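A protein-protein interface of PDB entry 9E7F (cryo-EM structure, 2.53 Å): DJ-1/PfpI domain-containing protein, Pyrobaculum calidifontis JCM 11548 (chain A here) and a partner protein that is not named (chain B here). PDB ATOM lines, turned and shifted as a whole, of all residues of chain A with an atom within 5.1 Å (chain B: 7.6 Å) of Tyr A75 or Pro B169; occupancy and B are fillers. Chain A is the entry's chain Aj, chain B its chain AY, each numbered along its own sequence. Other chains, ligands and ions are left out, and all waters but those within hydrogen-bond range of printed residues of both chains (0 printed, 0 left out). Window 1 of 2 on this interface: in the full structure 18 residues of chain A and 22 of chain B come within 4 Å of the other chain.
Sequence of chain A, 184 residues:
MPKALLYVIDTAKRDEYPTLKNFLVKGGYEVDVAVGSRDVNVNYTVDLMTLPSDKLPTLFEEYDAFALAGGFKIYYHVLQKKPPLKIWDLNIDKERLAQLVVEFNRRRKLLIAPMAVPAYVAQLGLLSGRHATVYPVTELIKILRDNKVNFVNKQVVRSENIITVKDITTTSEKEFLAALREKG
Among the printed residues, pairs that only touch across the chains: Phe A72 with Pro B169 (3.8 Å), Phe A72 with Leu B170 (3.6 Å), Tyr A75 with Pro B169 (3.4 Å), Tyr A76 with Gly B168 (3.1 Å), Tyr A76 with Pro B169 (3.6 Å), Trp A88 with Phe B158 (3.6 Å), Trp A88 with Arg B167 (3.7 Å), Trp A88 with Leu B170 (3.5 Å), Tyr A135 with Asn B172 (3.5 Å), Val A137 with Glu B68 (3.996 Å), Val A137 with Ile B69 (3.8 Å) and Glu A139 with Glu B68 (3.6 Å).
OE1 of Glu B68 lies close to OH of Tyr B166, at 3.2 Å. The backbone NH (N) of Glu B68 lies within hydrogen-bond range of the backbone carbonyl oxygen (O) of Gly B168 (3.4 Å). The backbone carbonyl oxygen (O) of Glu B68 sits at hydrogen-bond distance from the side-chain amide nitrogen (ND2) of Asn B172, 3.1 Å away. The backbone NH (N) of Thr B73 is in hydrogen-bond range of the side-chain carboxylate (OD2) of Asp B70 (2.6 Å). The side-chain hydroxyl (OG1) of Thr B73 lies close to the side-chain amide oxygen (OD1) of Asn B172 (3.4 Å). The side-chain amide nitrogen (ND2) of Asn B172 sits at hydrogen-bond distance from the backbone carbonyl oxygen (O) of Pro B169, 3.3 Å away.
OH of Tyr A75 sits at hydrogen-bond distance from OE1 of Glu B68 (3.1 Å). The side-chain hydroxyl (OH) of Tyr A135 lies within hydrogen-bond range of the side-chain carboxylate (OD1) of Asp B70, 3.4 Å away. The side-chain hydroxyl (OH) of Tyr A76 is in hydrogen-bond range of the side-chain hydroxyl (OH) of Tyr B166 (2.6 Å).
Hydrophobic or aromatic side chains of chain B that line the printed part of chain A: Phe B158, Tyr B166, Pro B169 and Leu B170. Of the 16 printed residues of chain A, 7 touch a printed residue of chain B. Among the printed residues, 15 pairs touch across the chains.
Of chain B, only Glu B68 and Pro B169 come within 4 Å of Tyr A75. Of the printed residues of chain A, Phe B158 touches Trp A88. Of the printed residues of chain A, Ile B69 touches Val A137 (3.8 Å). Of the printed residues of chain A, Glu B68 touches Tyr A75, Val A137 and Glu A139. Of the printed residues of chain A, Arg B167 touches Trp A88. Ile A74 touches none of the printed residues of chain B. The nearest residue of chain B that does not touch Tyr A75 is Tyr B166 (5.1 Å).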
ATOM      1  N   GLY A  71     -20.091 -29.095  -6.857  1.00  0.00           N
ATOM      2  CA  GLY A  71     -19.428 -27.813  -7.000  1.00  0.00           C
ATOM      3  C   GLY A  71     -19.263 -27.091  -5.684  1.00  0.00           C
ATOM      4  O   GLY A  71     -18.449 -27.490  -4.849  1.00  0.00           O
ATOM      5  N   PHE A  72     -20.021 -26.016  -5.488  1.00  0.00           N
ATOM      6  CA  PHE A  72     -19.960 -25.288  -4.231  1.00  0.00           C
ATOM      7  C   PHE A  72     -20.862 -25.880  -3.159  1.00  0.00           C
ATOM      8  O   PHE A  72     -20.731 -25.507  -1.990  1.00  0.00           O
ATOM      9  CB  PHE A  72     -20.312 -23.819  -4.459  1.00  0.00           C
ATOM     10  CG  PHE A  72     -19.551 -23.189  -5.583  1.00  0.00           C
ATOM     11  CD1 PHE A  72     -18.177 -23.079  -5.524  1.00  0.00           C
ATOM     12  CD2 PHE A  72     -20.208 -22.712  -6.699  1.00  0.00           C
ATOM     13  CE1 PHE A  72     -17.470 -22.502  -6.557  1.00  0.00           C
ATOM     14  CE2 PHE A  72     -19.506 -22.134  -7.734  1.00  0.00           C
ATOM     15  CZ  PHE A  72     -18.136 -22.029  -7.661  1.00  0.00           C
ATOM     16  N   LYS A  73     -21.774 -26.781  -3.524  1.00  0.00           N
ATOM     17  CA  LYS A  73     -22.535 -27.510  -2.515  1.00  0.00           C
ATOM     18  C   LYS A  73     -21.614 -28.361  -1.658  1.00  0.00           C
ATOM     19  O   LYS A  73     -21.724 -28.377  -0.427  1.00  0.00           O
ATOM     20  CB  LYS A  73     -23.587 -28.390  -3.188  1.00  0.00           C
ATOM     21  CG  LYS A  73     -24.922 -27.734  -3.409  1.00  0.00           C
ATOM     22  CD  LYS A  73     -25.842 -28.672  -4.152  1.00  0.00           C
ATOM     23  CE  LYS A  73     -26.979 -27.919  -4.804  1.00  0.00           C
ATOM     24  NZ  LYS A  73     -27.354 -28.517  -6.116  1.00  0.00           N
ATOM     25  N   ILE A  74     -20.698 -29.082  -2.298  1.00  0.00           N
ATOM     26  CA  ILE A  74     -19.793 -29.958  -1.567  1.00  0.00           C
ATOM     27  C   ILE A  74     -18.761 -29.144  -0.800  1.00  0.00           C
ATOM     28  O   ILE A  74     -18.324 -29.544   0.285  1.00  0.00           O
ATOM     29  CB  ILE A  74     -19.137 -30.959  -2.534  1.00  0.00           C
ATOM     30  CG1 ILE A  74     -20.102 -32.108  -2.826  1.00  0.00           C
ATOM     31  CG2 ILE A  74     -17.839 -31.493  -1.960  1.00  0.00           C
ATOM     32  CD1 ILE A  74     -20.652 -32.754  -1.588  1.00  0.00           C
ATOM     33  N   TYR A  75     -18.357 -27.993  -1.349  1.00  0.00           N
ATOM     34  CA  TYR A  75     -17.347 -27.157  -0.701  1.00  0.00           C
ATOM     35  C   TYR A  75     -17.851 -26.647   0.640  1.00  0.00           C
ATOM     36  O   TYR A  75     -17.113 -26.660   1.630  1.00  0.00           O
ATOM     37  CB  TYR A  75     -16.934 -26.028  -1.675  1.00  0.00           C
ATOM     38  CG  TYR A  75     -15.961 -24.896  -1.257  1.00  0.00           C
ATOM     39  CD1 TYR A  75     -16.218 -23.996  -0.217  1.00  0.00           C
ATOM     40  CD2 TYR A  75     -14.741 -24.775  -1.905  1.00  0.00           C
ATOM     41  CE1 TYR A  75     -15.326 -23.018   0.126  1.00  0.00           C
ATOM     42  CE2 TYR A  75     -13.838 -23.801  -1.557  1.00  0.00           C
ATOM     43  CZ  TYR A  75     -14.136 -22.925  -0.541  1.00  0.00           C
ATOM     44  OH  TYR A  75     -13.238 -21.942  -0.196  1.00  0.00           O
ATOM     45  N   TYR A  76     -19.091 -26.182   0.695  1.00  0.00           N
ATOM     46  CA  TYR A  76     -19.598 -25.647   1.947  1.00  0.00           C
ATOM     47  C   TYR A  76     -20.078 -26.732   2.894  1.00  0.00           C
ATOM     48  O   TYR A  76     -20.183 -26.480   4.097  1.00  0.00           O
ATOM     49  CB  TYR A  76     -20.705 -24.635   1.667  1.00  0.00           C
ATOM     50  CG  TYR A  76     -20.148 -23.310   1.213  1.00  0.00           C
ATOM     51  CD1 TYR A  76     -19.602 -22.423   2.122  1.00  0.00           C
ATOM     52  CD2 TYR A  76     -20.145 -22.960  -0.126  1.00  0.00           C
ATOM     53  CE1 TYR A  76     -19.080 -21.222   1.715  1.00  0.00           C
ATOM     54  CE2 TYR A  76     -19.628 -21.759  -0.541  1.00  0.00           C
ATOM     55  CZ  TYR A  76     -19.094 -20.893   0.384  1.00  0.00           C
ATOM     56  OH  TYR A  76     -18.572 -19.688  -0.021  1.00  0.00           O
ATOM     57  N   HIS A  77     -20.366 -27.930   2.389  1.00  0.00           N
ATOM     58  CA  HIS A  77     -20.676 -29.042   3.276  1.00  0.00           C
ATOM     59  C   HIS A  77     -19.428 -29.531   3.995  1.00  0.00           C
ATOM     60  O   HIS A  77     -19.469 -29.838   5.190  1.00  0.00           O
ATOM     61  CB  HIS A  77     -21.319 -30.184   2.494  1.00  0.00           C
ATOM     62  CG  HIS A  77     -21.569 -31.408   3.316  1.00  0.00           C
ATOM     63  ND1 HIS A  77     -21.296 -32.679   2.860  1.00  0.00           N
ATOM     64  CD2 HIS A  77     -22.063 -31.556   4.568  1.00  0.00           C
ATOM     65  CE1 HIS A  77     -21.607 -33.556   3.796  1.00  0.00           C
ATOM     66  NE2 HIS A  77     -22.074 -32.902   4.841  1.00  0.00           N
ATOM     67  N   VAL A  78     -18.309 -29.616   3.277  1.00  0.00           N
ATOM     68  CA  VAL A  78     -17.055 -30.050   3.887  1.00  0.00           C
ATOM     69  C   VAL A  78     -16.597 -29.049   4.938  1.00  0.00           C
ATOM     70  O   VAL A  78     -16.109 -29.428   6.008  1.00  0.00           O
ATOM     71  CB  VAL A  78     -15.984 -30.260   2.804  1.00  0.00           C
ATOM     72  CG1 VAL A  78     -14.607 -30.244   3.422  1.00  0.00           C
ATOM     73  CG2 VAL A  78     -16.232 -31.559   2.065  1.00  0.00           C
ATOM     74  N   LEU A  79     -16.741 -27.759   4.650  1.00  0.00           N
ATOM     75  CA  LEU A  79     -16.381 -26.718   5.598  1.00  0.00           C
ATOM     76  C   LEU A  79     -17.407 -26.548   6.705  1.00  0.00           C
ATOM     77  O   LEU A  79     -17.099 -25.908   7.714  1.00  0.00           O
ATOM     78  CB  LEU A  79     -16.204 -25.391   4.868  1.00  0.00           C
ATOM     79  CG  LEU A  79     -15.024 -25.370   3.910  1.00  0.00           C
ATOM     80  CD1 LEU A  79     -14.872 -23.993   3.318  1.00  0.00           C
ATOM     81  CD2 LEU A  79     -13.766 -25.794   4.635  1.00  0.00           C
ATOM     82  N   TRP A  88     -26.715 -22.957  -2.779  1.00  0.00           N
ATOM     83  CA  TRP A  88     -25.428 -23.614  -2.662  1.00  0.00           C
ATOM     84  C   TRP A  88     -25.422 -24.660  -1.561  1.00  0.00           C
ATOM     85  O   TRP A  88     -24.352 -25.142  -1.182  1.00  0.00           O
ATOM     86  CB  TRP A  88     -24.331 -22.585  -2.408  1.00  0.00           C
ATOM     87  CG  TRP A  88     -23.923 -21.855  -3.630  1.00  0.00           C
ATOM     88  CD1 TRP A  88     -24.479 -21.955  -4.865  1.00  0.00           C
ATOM     89  CD2 TRP A  88     -22.855 -20.917  -3.744  1.00  0.00           C
ATOM     90  NE1 TRP A  88     -23.832 -21.128  -5.743  1.00  0.00           N
ATOM     91  CE2 TRP A  88     -22.826 -20.480  -5.078  1.00  0.00           C
ATOM     92  CE3 TRP A  88     -21.916 -20.405  -2.846  1.00  0.00           C
ATOM     93  CZ2 TRP A  88     -21.898 -19.552  -5.538  1.00  0.00           C
ATOM     94  CZ3 TRP A  88     -20.997 -19.485  -3.300  1.00  0.00           C
ATOM     95  CH2 TRP A  88     -20.993 -19.067  -4.633  1.00  0.00           C
ATOM     96  N   MET A 115     -12.102 -30.648  -7.299  1.00  0.00           N
ATOM     97  CA  MET A 115     -12.390 -29.470  -6.473  1.00  0.00           C
ATOM     98  C   MET A 115     -12.456 -29.889  -5.010  1.00  0.00           C
ATOM     99  O   MET A 115     -11.490 -30.496  -4.519  1.00  0.00           O
ATOM    100  CB  MET A 115     -13.641 -28.782  -7.020  1.00  0.00           C
ATOM    101  CG  MET A 115     -13.345 -27.621  -7.951  1.00  0.00           C
ATOM    102  SD  MET A 115     -14.565 -26.298  -7.838  1.00  0.00           S
ATOM    103  CE  MET A 115     -14.354 -25.782  -6.136  1.00  0.00           C
ATOM    104  N   ALA A 116     -13.530 -29.596  -4.282  1.00  0.00           N
ATOM    105  CA  ALA A 116     -13.614 -29.919  -2.865  1.00  0.00           C
ATOM    106  C   ALA A 116     -14.065 -31.345  -2.605  1.00  0.00           C
ATOM    107  O   ALA A 116     -14.137 -31.744  -1.438  1.00  0.00           O
ATOM    108  CB  ALA A 116     -14.565 -28.955  -2.156  1.00  0.00           C
ATOM    109  N   TYR A 135      -8.771 -28.579  -4.044  1.00  0.00           N
ATOM    110  CA  TYR A 135      -8.815 -27.173  -4.397  1.00  0.00           C
ATOM    111  C   TYR A 135      -7.987 -26.375  -3.393  1.00  0.00           C
ATOM    112  O   TYR A 135      -8.286 -26.404  -2.191  1.00  0.00           O
ATOM    113  CB  TYR A 135     -10.255 -26.683  -4.407  1.00  0.00           C
ATOM    114  CG  TYR A 135     -10.485 -25.434  -5.217  1.00  0.00           C
ATOM    115  CD1 TYR A 135     -10.451 -25.465  -6.598  1.00  0.00           C
ATOM    116  CD2 TYR A 135     -10.760 -24.229  -4.595  1.00  0.00           C
ATOM    117  CE1 TYR A 135     -10.672 -24.332  -7.335  1.00  0.00           C
ATOM    118  CE2 TYR A 135     -10.983 -23.091  -5.322  1.00  0.00           C
ATOM    119  CZ  TYR A 135     -10.938 -23.144  -6.692  1.00  0.00           C
ATOM    120  OH  TYR A 135     -11.159 -22.004  -7.421  1.00  0.00           O
ATOM    121  N   VAL A 137      -7.335 -23.966  -1.378  1.00  0.00           N
ATOM    122  CA  VAL A 137      -7.658 -22.913  -0.432  1.00  0.00           C
ATOM    123  C   VAL A 137      -7.125 -23.338   0.927  1.00  0.00           C
ATOM    124  O   VAL A 137      -6.757 -24.495   1.143  1.00  0.00           O
ATOM    125  CB  VAL A 137      -9.169 -22.611  -0.366  1.00  0.00           C
ATOM    126  CG1 VAL A 137      -9.628 -21.939  -1.648  1.00  0.00           C
ATOM    127  CG2 VAL A 137      -9.957 -23.880  -0.105  1.00  0.00           C
ATOM    128  N   GLU A 139      -8.581 -23.589   3.926  1.00  0.00           N
ATOM    129  CA  GLU A 139      -9.376 -24.472   4.773  1.00  0.00           C
ATOM    130  C   GLU A 139      -9.413 -25.895   4.229  1.00  0.00           C
ATOM    131  O   GLU A 139      -9.336 -26.856   4.998  1.00  0.00           O
ATOM    132  CB  GLU A 139     -10.785 -23.910   4.923  1.00  0.00           C
ATOM    133  CG  GLU A 139     -10.808 -22.446   5.320  1.00  0.00           C
ATOM    134  CD  GLU A 139     -11.769 -21.635   4.479  1.00  0.00           C
ATOM    135  OE1 GLU A 139     -11.838 -21.878   3.257  1.00  0.00           O
ATOM    136  OE2 GLU A 139     -12.455 -20.756   5.037  1.00  0.00           O
ATOM    137  N   LEU A 140      -9.531 -26.051   2.909  1.00  0.00           N
ATOM    138  CA  LEU A 140      -9.585 -27.389   2.326  1.00  0.00           C
ATOM    139  C   LEU A 140      -8.252 -28.109   2.460  1.00  0.00           C
ATOM    140  O   LEU A 140      -8.218 -29.328   2.661  1.00  0.00           O
ATOM    141  CB  LEU A 140      -9.995 -27.310   0.857  1.00  0.00           C
ATOM    142  CG  LEU A 140     -11.415 -26.857   0.536  1.00  0.00           C
ATOM    143  CD1 LEU A 140     -11.632 -26.869  -0.964  1.00  0.00           C
ATOM    144  CD2 LEU A 140     -12.439 -27.727   1.236  1.00  0.00           C
ATOM    145  N   TYR B  14      -7.893 -14.531   2.393  1.00  0.00           N
ATOM    146  CA  TYR B  14      -8.964 -13.979   1.585  1.00  0.00           C
ATOM    147  C   TYR B  14      -8.420 -12.990   0.567  1.00  0.00           C
ATOM    148  O   TYR B  14      -7.398 -12.338   0.788  1.00  0.00           O
ATOM    149  CB  TYR B  14     -10.001 -13.284   2.464  1.00  0.00           C
ATOM    150  CG  TYR B  14     -10.827 -14.228   3.296  1.00  0.00           C
ATOM    151  CD1 TYR B  14     -11.791 -15.031   2.713  1.00  0.00           C
ATOM    152  CD2 TYR B  14     -10.648 -14.313   4.666  1.00  0.00           C
ATOM    153  CE1 TYR B  14     -12.547 -15.889   3.465  1.00  0.00           C
ATOM    154  CE2 TYR B  14     -11.398 -15.171   5.424  1.00  0.00           C
ATOM    155  CZ  TYR B  14     -12.351 -15.955   4.822  1.00  0.00           C
ATOM    156  OH  TYR B  14     -13.107 -16.813   5.583  1.00  0.00           O
ATOM    157  N   TRP B  66     -15.213 -10.263  -2.015  1.00  0.00           N
ATOM    158  CA  TRP B  66     -14.123 -11.011  -1.415  1.00  0.00           C
ATOM    159  C   TRP B  66     -14.477 -12.485  -1.351  1.00  0.00           C
ATOM    160  O   TRP B  66     -15.639 -12.875  -1.480  1.00  0.00           O
ATOM    161  CB  TRP B  66     -13.784 -10.486  -0.016  1.00  0.00           C
ATOM    162  CG  TRP B  66     -14.915 -10.541   0.963  1.00  0.00           C
ATOM    163  CD1 TRP B  66     -15.977  -9.697   1.033  1.00  0.00           C
ATOM    164  CD2 TRP B  66     -15.086 -11.483   2.022  1.00  0.00           C
ATOM    165  NE1 TRP B  66     -16.802 -10.056   2.061  1.00  0.00           N
ATOM    166  CE2 TRP B  66     -16.273 -11.150   2.688  1.00  0.00           C
ATOM    167  CE3 TRP B  66     -14.347 -12.577   2.473  1.00  0.00           C
ATOM    168  CZ2 TRP B  66     -16.742 -11.873   3.774  1.00  0.00           C
ATOM    169  CZ3 TRP B  66     -14.810 -13.288   3.548  1.00  0.00           C
ATOM    170  CH2 TRP B  66     -15.996 -12.937   4.188  1.00  0.00           C
ATOM    171  N   GLY B  67     -13.452 -13.299  -1.145  1.00  0.00           N
ATOM    172  CA  GLY B  67     -13.640 -14.732  -1.042  1.00  0.00           C
ATOM    173  C   GLY B  67     -12.324 -15.405  -0.742  1.00  0.00           C
ATOM    174  O   GLY B  67     -11.278 -14.759  -0.634  1.00  0.00           O
ATOM    175  N   GLU B  68     -12.391 -16.725  -0.609  1.00  0.00           N
ATOM    176  CA  GLU B  68     -11.209 -17.527  -0.320  1.00  0.00           C
ATOM    177  C   GLU B  68     -10.388 -17.690  -1.589  1.00  0.00           C
ATOM    178  O   GLU B  68     -10.868 -18.255  -2.575  1.00  0.00           O
ATOM    179  CB  GLU B  68     -11.613 -18.887   0.238  1.00  0.00           C
ATOM    180  CG  GLU B  68     -12.516 -18.806   1.454  1.00  0.00           C
ATOM    181  CD  GLU B  68     -13.982 -18.971   1.107  1.00  0.00           C
ATOM    182  OE1 GLU B  68     -14.298 -19.040  -0.095  1.00  0.00           O
ATOM    183  OE2 GLU B  68     -14.819 -19.021   2.032  1.00  0.00           O
ATOM    184  N   ILE B  69      -9.154 -17.203  -1.563  1.00  0.00           N
ATOM    185  CA  ILE B  69      -8.270 -17.278  -2.720  1.00  0.00           C
ATOM    186  C   ILE B  69      -7.529 -18.607  -2.702  1.00  0.00           C
ATOM    187  O   ILE B  69      -7.126 -19.096  -1.641  1.00  0.00           O
ATOM    188  CB  ILE B  69      -7.297 -16.085  -2.732  1.00  0.00           C
ATOM    189  CG1 ILE B  69      -6.339 -16.187  -3.914  1.00  0.00           C
ATOM    190  CG2 ILE B  69      -6.513 -16.010  -1.439  1.00  0.00           C
ATOM    191  CD1 ILE B  69      -5.849 -14.863  -4.407  1.00  0.00           C
ATOM    192  N   ASP B  70      -7.359 -19.208  -3.874  1.00  0.00           N
ATOM    193  CA  ASP B  70      -6.659 -20.477  -3.992  1.00  0.00           C
ATOM    194  C   ASP B  70      -5.195 -20.244  -4.334  1.00  0.00           C
ATOM    195  O   ASP B  70      -4.803 -19.174  -4.804  1.00  0.00           O
ATOM    196  CB  ASP B  70      -7.364 -21.394  -5.013  1.00  0.00           C
ATOM    197  CG  ASP B  70      -7.026 -21.089  -6.481  1.00  0.00           C
ATOM    198  OD1 ASP B  70      -7.968 -20.729  -7.213  1.00  0.00           O
ATOM    199  OD2 ASP B  70      -5.893 -21.324  -6.960  1.00  0.00           O
ATOM    200  N   THR B  73      -4.493 -19.603  -8.221  1.00  0.00           N
ATOM    201  CA  THR B  73      -4.864 -18.276  -8.698  1.00  0.00           C
ATOM    202  C   THR B  73      -3.903 -17.216  -8.183  1.00  0.00           C
ATOM    203  O   THR B  73      -3.565 -16.276  -8.906  1.00  0.00           O
ATOM    204  CB  THR B  73      -6.292 -17.945  -8.281  1.00  0.00           C
ATOM    205  OG1 THR B  73      -7.191 -18.889  -8.873  1.00  0.00           O
ATOM    206  CG2 THR B  73      -6.659 -16.546  -8.736  1.00  0.00           C
ATOM    207  N   PHE B 158     -23.845  -9.913  -4.024  1.00  0.00           N
ATOM    208  CA  PHE B 158     -23.723 -11.185  -4.727  1.00  0.00           C
ATOM    209  C   PHE B 158     -24.844 -12.142  -4.351  1.00  0.00           C
ATOM    210  O   PHE B 158     -25.259 -12.966  -5.171  1.00  0.00           O
ATOM    211  CB  PHE B 158     -22.359 -11.807  -4.424  1.00  0.00           C
ATOM    212  CG  PHE B 158     -22.179 -13.201  -4.963  1.00  0.00           C
ATOM    213  CD1 PHE B 158     -21.831 -13.405  -6.283  1.00  0.00           C
ATOM    214  CD2 PHE B 158     -22.326 -14.304  -4.138  1.00  0.00           C
ATOM    215  CE1 PHE B 158     -21.657 -14.678  -6.772  1.00  0.00           C
ATOM    216  CE2 PHE B 158     -22.156 -15.574  -4.623  1.00  0.00           C
ATOM    217  CZ  PHE B 158     -21.820 -15.764  -5.940  1.00  0.00           C
ATOM    218  N   TYR B 166     -19.540 -11.188   0.306  1.00  0.00           N
ATOM    219  CA  TYR B 166     -18.793 -12.434   0.319  1.00  0.00           C
ATOM    220  C   TYR B 166     -19.171 -13.285  -0.882  1.00  0.00           C
ATOM    221  O   TYR B 166     -20.349 -13.564  -1.121  1.00  0.00           O
ATOM    222  CB  TYR B 166     -19.058 -13.193   1.612  1.00  0.00           C
ATOM    223  CG  TYR B 166     -18.510 -14.592   1.606  1.00  0.00           C
ATOM    224  CD1 TYR B 166     -17.150 -14.821   1.516  1.00  0.00           C
ATOM    225  CD2 TYR B 166     -19.355 -15.689   1.680  1.00  0.00           C
ATOM    226  CE1 TYR B 166     -16.646 -16.093   1.509  1.00  0.00           C
ATOM    227  CE2 TYR B 166     -18.861 -16.965   1.669  1.00  0.00           C
ATOM    228  CZ  TYR B 166     -17.505 -17.165   1.585  1.00  0.00           C
ATOM    229  OH  TYR B 166     -16.999 -18.440   1.572  1.00  0.00           O
ATOM    230  N   ARG B 167     -18.161 -13.713  -1.627  1.00  0.00           N
ATOM    231  CA  ARG B 167     -18.354 -14.386  -2.897  1.00  0.00           C
ATOM    232  C   ARG B 167     -18.042 -15.872  -2.847  1.00  0.00           C
ATOM    233  O   ARG B 167     -18.417 -16.596  -3.772  1.00  0.00           O
ATOM    234  CB  ARG B 167     -17.481 -13.712  -3.962  1.00  0.00           C
ATOM    235  CG  ARG B 167     -17.746 -14.131  -5.373  1.00  0.00           C
ATOM    236  CD  ARG B 167     -16.871 -13.348  -6.326  1.00  0.00           C
ATOM    237  NE  ARG B 167     -17.374 -11.998  -6.523  1.00  0.00           N
ATOM    238  CZ  ARG B 167     -17.947 -11.577  -7.638  1.00  0.00           C
ATOM    239  NH1 ARG B 167     -18.099 -12.375  -8.680  1.00  0.00           N
ATOM    240  NH2 ARG B 167     -18.376 -10.323  -7.712  1.00  0.00           N
ATOM    241  N   GLY B 168     -17.387 -16.347  -1.797  1.00  0.00           N
ATOM    242  CA  GLY B 168     -16.972 -17.724  -1.723  1.00  0.00           C
ATOM    243  C   GLY B 168     -15.754 -17.974  -2.583  1.00  0.00           C
ATOM    244  O   GLY B 168     -14.922 -17.089  -2.789  1.00  0.00           O
ATOM    245  N   PRO B 169     -15.633 -19.190  -3.120  1.00  0.00           N
ATOM    246  CA  PRO B 169     -14.511 -19.498  -4.014  1.00  0.00           C
ATOM    247  C   PRO B 169     -14.671 -18.933  -5.410  1.00  0.00           C
ATOM    248  O   PRO B 169     -13.774 -19.116  -6.238  1.00  0.00           O
ATOM    249  CB  PRO B 169     -14.502 -21.033  -4.052  1.00  0.00           C
ATOM    250  CG  PRO B 169     -15.637 -21.481  -3.196  1.00  0.00           C
ATOM    251  CD  PRO B 169     -16.535 -20.334  -2.957  1.00  0.00           C
ATOM    252  N   LEU B 170     -15.781 -18.258  -5.705  1.00  0.00           N
ATOM    253  CA  LEU B 170     -15.985 -17.631  -7.002  1.00  0.00           C
ATOM    254  C   LEU B 170     -15.142 -16.378  -7.193  1.00  0.00           C
ATOM    255  O   LEU B 170     -15.116 -15.837  -8.300  1.00  0.00           O
ATOM    256  CB  LEU B 170     -17.461 -17.295  -7.189  1.00  0.00           C
ATOM    257  CG  LEU B 170     -18.328 -18.407  -7.773  1.00  0.00           C
ATOM    258  CD1 LEU B 170     -19.774 -17.977  -7.807  1.00  0.00           C
ATOM    259  CD2 LEU B 170     -17.852 -18.765  -9.161  1.00  0.00           C
ATOM    260  N   ILE B 171     -14.463 -15.903  -6.146  1.00  0.00           N
ATOM    261  CA  ILE B 171     -13.537 -14.788  -6.275  1.00  0.00           C
ATOM    262  C   ILE B 171     -12.352 -15.138  -7.160  1.00  0.00           C
ATOM    263  O   ILE B 171     -11.726 -14.243  -7.733  1.00  0.00           O
ATOM    264  CB  ILE B 171     -13.064 -14.329  -4.880  1.00  0.00           C
ATOM    265  CG1 ILE B 171     -12.451 -12.935  -4.958  1.00  0.00           C
ATOM    266  CG2 ILE B 171     -12.081 -15.318  -4.297  1.00  0.00           C
ATOM    267  CD1 ILE B 171     -13.469 -11.838  -5.060  1.00  0.00           C
ATOM    268  N   ASN B 172     -12.014 -16.422  -7.275  1.00  0.00           N
ATOM    269  CA  ASN B 172     -10.938 -16.833  -8.165  1.00  0.00           C
ATOM    270  C   ASN B 172     -11.347 -16.760  -9.628  1.00  0.00           C
ATOM    271  O   ASN B 172     -10.509 -16.464 -10.485  1.00  0.00           O
ATOM    272  CB  ASN B 172     -10.482 -18.244  -7.814  1.00  0.00           C
ATOM    273  CG  ASN B 172      -9.883 -18.325  -6.437  1.00  0.00           C
ATOM    274  OD1 ASN B 172      -8.870 -17.690  -6.148  1.00  0.00           O
ATOM    275  ND2 ASN B 172     -10.515 -19.094  -5.566  1.00  0.00           N
ATOM    276  N   ASP B 173     -12.611 -17.042  -9.936  1.00  0.00           N
ATOM    277  CA  ASP B 173     -13.087 -16.880 -11.303  1.00  0.00           C
ATOM    278  C   ASP B 173     -13.073 -15.418 -11.719  1.00  0.00           C
ATOM    279  O   ASP B 173     -12.709 -15.094 -12.854  1.00  0.00           O
ATOM    280  CB  ASP B 173     -14.492 -17.464 -11.438  1.00  0.00           C
ATOM    281  CG  ASP B 173     -14.580 -18.883 -10.926  1.00  0.00           C
ATOM    282  OD1 ASP B 173     -14.895 -19.785 -11.729  1.00  0.00           O
ATOM    283  OD2 ASP B 173     -14.331 -19.098  -9.722  1.00  0.00           O
ATOM    284  N   LEU B 174     -13.481 -14.526 -10.819  1.00  0.00           N
ATOM    285  CA  LEU B 174     -13.438 -13.100 -11.114  1.00  0.00           C
ATOM    286  C   LEU B 174     -12.005 -12.617 -11.276  1.00  0.00           C
ATOM    287  O   LEU B 174     -11.721 -11.774 -12.132  1.00  0.00           O
ATOM    288  CB  LEU B 174     -14.146 -12.319 -10.013  1.00  0.00           C
ATOM    289  CG  LEU B 174     -14.198 -10.804 -10.186  1.00  0.00           C
ATOM    290  CD1 LEU B 174     -14.973 -10.432 -11.429  1.00  0.00           C
ATOM    291  CD2 LEU B 174     -14.802 -10.146  -8.963  1.00  0.00           C
